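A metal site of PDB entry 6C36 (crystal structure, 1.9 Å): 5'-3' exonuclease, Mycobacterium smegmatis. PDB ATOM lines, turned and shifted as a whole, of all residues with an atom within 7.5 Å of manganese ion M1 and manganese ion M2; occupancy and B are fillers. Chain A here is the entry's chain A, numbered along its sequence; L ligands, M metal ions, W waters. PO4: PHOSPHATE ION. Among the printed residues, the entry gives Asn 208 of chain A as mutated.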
ATOM      1  N   ASP A   9      10.964  10.191  -5.064  1.00  0.00           N
ATOM      2  CA  ASP A   9      11.805   8.989  -5.091  1.00  0.00           C
ATOM      3  C   ASP A   9      12.032   8.656  -6.570  1.00  0.00           C
ATOM      4  O   ASP A   9      11.222   7.983  -7.203  1.00  0.00           O
ATOM      5  CB  ASP A   9      11.116   7.854  -4.346  1.00  0.00           C
ATOM      6  CG  ASP A   9      11.976   6.607  -4.185  1.00  0.00           C
ATOM      7  OD1 ASP A   9      13.047   6.471  -4.815  1.00  0.00           O
ATOM      8  OD2 ASP A   9      11.528   5.729  -3.419  1.00  0.00           O
ATOM      9  N   ALA A  11      13.989   6.717  -8.512  1.00  0.00           N
ATOM     10  CA  ALA A  11      14.047   5.357  -9.060  1.00  0.00           C
ATOM     11  C   ALA A  11      12.729   4.637  -8.878  1.00  0.00           C
ATOM     12  O   ALA A  11      12.335   3.844  -9.744  1.00  0.00           O
ATOM     13  CB  ALA A  11      15.184   4.582  -8.401  1.00  0.00           C
ATOM     14  N   SER A  12      12.032   4.864  -7.765  1.00  0.00           N
ATOM     15  CA  SER A  12      10.696   4.274  -7.625  1.00  0.00           C
ATOM     16  C   SER A  12       9.802   4.721  -8.770  1.00  0.00           C
ATOM     17  O   SER A  12       9.102   3.908  -9.384  1.00  0.00           O
ATOM     18  CB  SER A  12      10.089   4.660  -6.273  1.00  0.00           C
ATOM     19  OG  SER A  12       8.750   4.190  -6.173  1.00  0.00           O
ATOM     20  N   ASP A  60      19.712   7.811  -6.043  1.00  0.00           N
ATOM     21  CA  ASP A  60      20.407   6.714  -5.383  1.00  0.00           C
ATOM     22  C   ASP A  60      21.881   6.793  -5.740  1.00  0.00           C
ATOM     23  O   ASP A  60      22.353   6.136  -6.674  1.00  0.00           O
ATOM     24  CB  ASP A  60      19.833   5.369  -5.826  1.00  0.00           C
ATOM     25  CG  ASP A  60      18.516   5.042  -5.137  1.00  0.00           C
ATOM     26  OD1 ASP A  60      17.443   5.225  -5.769  1.00  0.00           O
ATOM     27  OD2 ASP A  60      18.575   4.603  -3.977  1.00  0.00           O
ATOM     28  N   TRP A  63      22.583   2.593  -4.519  1.00  0.00           N
ATOM     29  CA  TRP A  63      21.324   1.908  -4.269  1.00  0.00           C
ATOM     30  C   TRP A  63      21.452   0.750  -3.293  1.00  0.00           C
ATOM     31  O   TRP A  63      20.435   0.276  -2.778  1.00  0.00           O
ATOM     32  CB  TRP A  63      20.742   1.365  -5.587  1.00  0.00           C
ATOM     33  CG  TRP A  63      21.535   0.172  -6.092  1.00  0.00           C
ATOM     34  CD1 TRP A  63      22.770   0.209  -6.679  1.00  0.00           C
ATOM     35  CD2 TRP A  63      21.173  -1.211  -5.996  1.00  0.00           C
ATOM     36  NE1 TRP A  63      23.182  -1.061  -6.994  1.00  0.00           N
ATOM     37  CE2 TRP A  63      22.223  -1.956  -6.573  1.00  0.00           C
ATOM     38  CE3 TRP A  63      20.051  -1.884  -5.490  1.00  0.00           C
ATOM     39  CZ2 TRP A  63      22.183  -3.349  -6.656  1.00  0.00           C
ATOM     40  CZ3 TRP A  63      20.023  -3.271  -5.562  1.00  0.00           C
ATOM     41  CH2 TRP A  63      21.086  -3.988  -6.141  1.00  0.00           C
ATOM     42  N   TYR A  75      20.914  -8.340   2.242  1.00  0.00           N
ATOM     43  CA  TYR A  75      20.229  -7.110   1.863  1.00  0.00           C
ATOM     44  C   TYR A  75      20.363  -6.843   0.375  1.00  0.00           C
ATOM     45  O   TYR A  75      21.473  -6.680  -0.137  1.00  0.00           O
ATOM     46  CB  TYR A  75      20.815  -5.937   2.657  1.00  0.00           C
ATOM     47  CG  TYR A  75      20.127  -4.608   2.422  1.00  0.00           C
ATOM     48  CD1 TYR A  75      18.827  -4.399   2.870  1.00  0.00           C
ATOM     49  CD2 TYR A  75      20.794  -3.565   1.780  1.00  0.00           C
ATOM     50  CE1 TYR A  75      18.201  -3.179   2.669  1.00  0.00           C
ATOM     51  CE2 TYR A  75      20.187  -2.339   1.574  1.00  0.00           C
ATOM     52  CZ  TYR A  75      18.887  -2.159   2.031  1.00  0.00           C
ATOM     53  OH  TYR A  75      18.273  -0.932   1.841  1.00  0.00           O
ATOM     54  N   LYS A  76      19.205  -6.816  -0.311  1.00  0.00           N
ATOM     55  CA  LYS A  76      19.086  -6.606  -1.762  1.00  0.00           C
ATOM     56  C   LYS A  76      19.945  -7.569  -2.580  1.00  0.00           C
ATOM     57  O   LYS A  76      20.172  -7.337  -3.784  1.00  0.00           O
ATOM     58  CB  LYS A  76      19.398  -5.157  -2.143  1.00  0.00           C
ATOM     59  CG  LYS A  76      18.527  -4.118  -1.411  1.00  0.00           C
ATOM     60  CD  LYS A  76      18.679  -2.730  -2.030  1.00  0.00           C
ATOM     61  CE  LYS A  76      17.701  -1.725  -1.418  1.00  0.00           C
ATOM     62  NZ  LYS A  76      17.725  -0.388  -2.135  1.00  0.00           N
ATOM     63  N   ARG A  79      18.871  -8.843  -6.051  1.00  0.00           N
ATOM     64  CA  ARG A  79      18.698  -7.834  -7.082  1.00  0.00           C
ATOM     65  C   ARG A  79      20.018  -7.384  -7.701  1.00  0.00           C
ATOM     66  O   ARG A  79      20.022  -6.457  -8.510  1.00  0.00           O
ATOM     67  CB  ARG A  79      17.979  -6.607  -6.502  1.00  0.00           C
ATOM     68  CG  ARG A  79      16.576  -6.883  -5.969  1.00  0.00           C
ATOM     69  CD  ARG A  79      15.773  -5.591  -5.980  1.00  0.00           C
ATOM     70  NE  ARG A  79      15.474  -5.082  -4.664  1.00  0.00           N
ATOM     71  CZ  ARG A  79      15.568  -3.797  -4.322  1.00  0.00           C
ATOM     72  NH1 ARG A  79      15.979  -2.897  -5.208  1.00  0.00           N
ATOM     73  NH2 ARG A  79      15.256  -3.425  -3.092  1.00  0.00           N
ATOM     74  N   GLU A 123      21.184   5.705  -0.113  1.00  0.00           N
ATOM     75  CA  GLU A 123      20.068   5.507  -1.019  1.00  0.00           C
ATOM     76  C   GLU A 123      19.218   6.770  -1.125  1.00  0.00           C
ATOM     77  O   GLU A 123      19.298   7.679  -0.305  1.00  0.00           O
ATOM     78  CB  GLU A 123      19.191   4.348  -0.539  1.00  0.00           C
ATOM     79  CG  GLU A 123      19.941   3.055  -0.310  1.00  0.00           C
ATOM     80  CD  GLU A 123      19.042   1.912   0.102  1.00  0.00           C
ATOM     81  OE1 GLU A 123      19.486   1.075   0.920  1.00  0.00           O
ATOM     82  OE2 GLU A 123      17.914   1.822  -0.430  1.00  0.00           O
ATOM     83  N   ALA A 124      18.407   6.821  -2.190  1.00  0.00           N
ATOM     84  CA  ALA A 124      17.397   7.871  -2.240  1.00  0.00           C
ATOM     85  C   ALA A 124      16.477   7.821  -1.020  1.00  0.00           C
ATOM     86  O   ALA A 124      15.993   8.866  -0.571  1.00  0.00           O
ATOM     87  CB  ALA A 124      16.577   7.764  -3.527  1.00  0.00           C
ATOM     88  N   ASP A 125      16.229   6.622  -0.473  1.00  0.00           N
ATOM     89  CA  ASP A 125      15.462   6.508   0.769  1.00  0.00           C
ATOM     90  C   ASP A 125      16.085   7.377   1.864  1.00  0.00           C
ATOM     91  O   ASP A 125      15.362   8.046   2.628  1.00  0.00           O
ATOM     92  CB  ASP A 125      15.418   5.056   1.231  1.00  0.00           C
ATOM     93  CG  ASP A 125      14.921   4.106   0.159  1.00  0.00           C
ATOM     94  OD1 ASP A 125      14.189   3.166   0.493  1.00  0.00           O
ATOM     95  OD2 ASP A 125      15.250   4.339  -1.026  1.00  0.00           O
ATOM     96  N   ASP A 126      17.409   7.352   1.977  1.00  0.00           N
ATOM     97  CA  ASP A 126      18.104   8.132   3.003  1.00  0.00           C
ATOM     98  C   ASP A 126      18.049   9.631   2.708  1.00  0.00           C
ATOM     99  O   ASP A 126      17.881  10.445   3.627  1.00  0.00           O
ATOM    100  CB  ASP A 126      19.553   7.664   3.091  1.00  0.00           C
ATOM    101  CG  ASP A 126      19.649   6.191   3.409  1.00  0.00           C
ATOM    102  OD1 ASP A 126      18.993   5.769   4.390  1.00  0.00           O
ATOM    103  OD2 ASP A 126      20.363   5.473   2.681  1.00  0.00           O
ATOM    104  N   LEU A 128      15.664  11.133   1.103  1.00  0.00           N
ATOM    105  CA  LEU A 128      14.291  11.517   1.426  1.00  0.00           C
ATOM    106  C   LEU A 128      14.078  11.638   2.925  1.00  0.00           C
ATOM    107  O   LEU A 128      13.431  12.570   3.403  1.00  0.00           O
ATOM    108  CB  LEU A 128      13.315  10.497   0.836  1.00  0.00           C
ATOM    109  CG  LEU A 128      13.212  10.482  -0.689  1.00  0.00           C
ATOM    110  CD1 LEU A 128      12.740   9.118  -1.175  1.00  0.00           C
ATOM    111  CD2 LEU A 128      12.267  11.562  -1.168  1.00  0.00           C
ATOM    112  N   SER A 144       6.463   8.148  -3.693  1.00  0.00           N
ATOM    113  CA  SER A 144       7.202   6.900  -3.839  1.00  0.00           C
ATOM    114  C   SER A 144       6.255   5.720  -3.870  1.00  0.00           C
ATOM    115  O   SER A 144       5.202   5.738  -3.217  1.00  0.00           O
ATOM    116  CB  SER A 144       8.205   6.704  -2.693  1.00  0.00           C
ATOM    117  OG  SER A 144       8.992   5.535  -2.899  1.00  0.00           O
ATOM    118  N   ASP A 146       7.568   2.952  -2.674  1.00  0.00           N
ATOM    119  CA  ASP A 146       8.356   2.117  -1.767  1.00  0.00           C
ATOM    120  C   ASP A 146       7.769   2.252  -0.372  1.00  0.00           C
ATOM    121  O   ASP A 146       7.882   3.314   0.251  1.00  0.00           O
ATOM    122  CB  ASP A 146       9.817   2.551  -1.805  1.00  0.00           C
ATOM    123  CG  ASP A 146      10.724   1.703  -0.907  1.00  0.00           C
ATOM    124  OD1 ASP A 146      10.251   0.747  -0.248  1.00  0.00           O
ATOM    125  OD2 ASP A 146      11.936   2.017  -0.883  1.00  0.00           O
ATOM    126  N   ARG A 147       7.186   1.173   0.138  1.00  0.00           N
ATOM    127  CA  ARG A 147       6.572   1.230   1.463  1.00  0.00           C
ATOM    128  C   ARG A 147       7.568   1.506   2.576  1.00  0.00           C
ATOM    129  O   ARG A 147       7.149   1.902   3.669  1.00  0.00           O
ATOM    130  CB  ARG A 147       5.789  -0.054   1.745  1.00  0.00           C
ATOM    131  CG  ARG A 147       4.423  -0.042   1.114  1.00  0.00           C
ATOM    132  CD  ARG A 147       3.685  -1.344   1.342  1.00  0.00           C
ATOM    133  NE  ARG A 147       4.601  -2.484   1.344  1.00  0.00           N
ATOM    134  CZ  ARG A 147       4.215  -3.740   1.535  1.00  0.00           C
ATOM    135  NH1 ARG A 147       2.934  -4.020   1.744  1.00  0.00           N
ATOM    136  NH2 ARG A 147       5.110  -4.715   1.518  1.00  0.00           N
ATOM    137  N   ASP A 148       8.881   1.316   2.329  1.00  0.00           N
ATOM    138  CA  ASP A 148       9.886   1.706   3.319  1.00  0.00           C
ATOM    139  C   ASP A 148       9.642   3.115   3.826  1.00  0.00           C
ATOM    140  O   ASP A 148       9.800   3.392   5.024  1.00  0.00           O
ATOM    141  CB  ASP A 148      11.313   1.645   2.741  1.00  0.00           C
ATOM    142  CG  ASP A 148      11.787   0.234   2.418  1.00  0.00           C
ATOM    143  OD1 ASP A 148      11.183  -0.759   2.902  1.00  0.00           O
ATOM    144  OD2 ASP A 148      12.788   0.133   1.679  1.00  0.00           O
ATOM    145  N   LEU A 149       9.271   4.037   2.928  1.00  0.00           N
ATOM    146  CA  LEU A 149       9.209   5.431   3.289  1.00  0.00           C
ATOM    147  C   LEU A 149       7.992   5.770   4.133  1.00  0.00           C
ATOM    148  O   LEU A 149       7.896   6.901   4.602  1.00  0.00           O
ATOM    149  CB  LEU A 149       9.258   6.292   2.030  1.00  0.00           C
ATOM    150  CG  LEU A 149      10.587   6.044   1.312  1.00  0.00           C
ATOM    151  CD1 LEU A 149      10.500   6.463  -0.105  1.00  0.00           C
ATOM    152  CD2 LEU A 149      11.714   6.789   2.013  1.00  0.00           C
ATOM    153  N   ASP A 205      11.155  -8.392   4.955  1.00  0.00           N
ATOM    154  CA  ASP A 205      10.952  -7.568   3.757  1.00  0.00           C
ATOM    155  C   ASP A 205      11.552  -8.296   2.569  1.00  0.00           C
ATOM    156  O   ASP A 205      12.740  -8.125   2.250  1.00  0.00           O
ATOM    157  CB  ASP A 205      11.583  -6.189   3.914  1.00  0.00           C
ATOM    158  CG  ASP A 205      11.001  -5.166   2.979  1.00  0.00           C
ATOM    159  OD1 ASP A 205      10.681  -5.513   1.821  1.00  0.00           O
ATOM    160  OD2 ASP A 205      10.864  -4.004   3.410  1.00  0.00           O
ATOM    161  N   ASN A 208      13.475  -6.334  -0.128  1.00  0.00           N
ATOM    162  CA  ASN A 208      14.809  -5.878   0.245  1.00  0.00           C
ATOM    163  C   ASN A 208      15.743  -7.014   0.660  1.00  0.00           C
ATOM    164  O   ASN A 208      16.884  -6.748   1.066  1.00  0.00           O
ATOM    165  CB  ASN A 208      14.729  -4.868   1.400  1.00  0.00           C
ATOM    166  CG  ASN A 208      14.399  -3.476   0.914  1.00  0.00           C
ATOM    167  OD1 ASN A 208      14.481  -3.177  -0.276  1.00  0.00           O
ATOM    168  ND2 ASN A 208      14.023  -2.602   1.845  1.00  0.00           N
ATOM    169  N   VAL A 267      17.238  -1.066   8.430  1.00  0.00           N
ATOM    170  CA  VAL A 267      15.850  -0.832   8.010  1.00  0.00           C
ATOM    171  C   VAL A 267      15.498   0.635   8.117  1.00  0.00           C
ATOM    172  O   VAL A 267      14.779   1.179   7.272  1.00  0.00           O
ATOM    173  CB  VAL A 267      14.894  -1.713   8.842  1.00  0.00           C
ATOM    174  CG1 VAL A 267      13.453  -1.287   8.652  1.00  0.00           C
ATOM    175  CG2 VAL A 267      15.079  -3.175   8.464  1.00  0.00           C
ATOM    176  N   VAL A 269      15.775   4.484   7.680  1.00  0.00           N
ATOM    177  CA  VAL A 269      16.434   5.376   6.746  1.00  0.00           C
ATOM    178  C   VAL A 269      17.252   6.378   7.540  1.00  0.00           C
ATOM    179  O   VAL A 269      16.901   6.752   8.665  1.00  0.00           O
ATOM    180  CB  VAL A 269      15.423   6.076   5.819  1.00  0.00           C
ATOM    181  CG1 VAL A 269      14.607   5.049   5.046  1.00  0.00           C
ATOM    182  CG2 VAL A 269      14.529   6.982   6.644  1.00  0.00           C
HETATM  183  P   PO4 L   1      14.118  -0.121  -2.593  1.00  0.00           P
HETATM  184  O1  PO4 L   1      14.548   1.245  -2.101  1.00  0.00           O
HETATM  185  O2  PO4 L   1      13.507  -0.889  -1.412  1.00  0.00           O
HETATM  186  O3  PO4 L   1      15.320  -0.805  -3.175  1.00  0.00           O
HETATM  187  O4  PO4 L   1      13.084   0.017  -3.673  1.00  0.00           O
HETATM  188 MN    MN M   1      13.711   1.130  -0.080  1.00  0.00          MN
HETATM  189 MN    MN M   2      14.937   3.085  -2.953  1.00  0.00          MN
HETATM  190  O   HOH W   1      14.742   1.760  -4.798  1.00  0.00           O
HETATM  191  O   HOH W   2      15.799   0.654   0.912  1.00  0.00           O
HETATM  192  O   HOH W   3      17.187   2.705  -2.944  1.00  0.00           O
HETATM  193  O   HOH W   4      15.098   4.710  -4.360  1.00  0.00           O
HETATM  194  O   HOH W   5      12.831   3.366  -2.809  1.00  0.00           O
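The side-chain hydroxyl (OG) of Ser 144 sits at hydrogen-bond distance from the backbone NH (N) of Asp 146, 3.0 Å away.
OD2 of Asp 148 sits close to ND2 of Asn 208 (3.0 Å).
Three residues have an atom within 4 Å of manganese ion M1: Asp 125, Asp 146 and Asp 148.
The nearest printed residue that does not touch manganese ion M1 is Asn 208 (4.2 Å).
Within 4 Å of manganese ion M2: Asp 125 and Asp 146.
The nearest printed residue that does not touch manganese ion M2 is Asp 60 (4.1 Å).
Manganese ion M1 is bound by the side-chain carboxylate of Asp 146 (2.1 Å), the side-chain carboxylate of Asp 125 (2.2 Å), an oxygen (O1) of the ligand (2.2 Å), the side-chain carboxylate of Asp 148 (2.2 Å), water W2 (2.4 Å) and an oxygen (O2) of the ligand (2.4 Å).
O1 of the ligand is bound to manganese ion M2, 2.1 Å away.
Water W5 is bound to manganese ion M2, 2.1 Å away.
Manganese ion M2 is bound by water W4.
Water W1 binds manganese ion M2 (2.3 Å).
Water W3 is bound to manganese ion M2 (2.3 Å).
OD2 of Asp 125 binds manganese ion M2, 2.3 Å away.
Water W2 bridges the side-chain carboxylate (OE2) of Glu 123 (2.8 Å) and the side-chain hydroxyl (OH) of Tyr 75 (3.1 Å).
Water W4 lies within hydrogen-bond range of the side-chain carboxylate of Asp 9 (2.7 Å) and the side-chain carboxylate of Asp 60 (2.8 Å).
Water W3 lies within hydrogen-bond range of the side-chain carboxylate (OD2) of Asp 60 (2.6 Å), the side-chain carboxylate (OE2) of Glu 123 (2.8 Å) and the side-chain amino group (NZ) of Lys 76 (3.2 Å).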
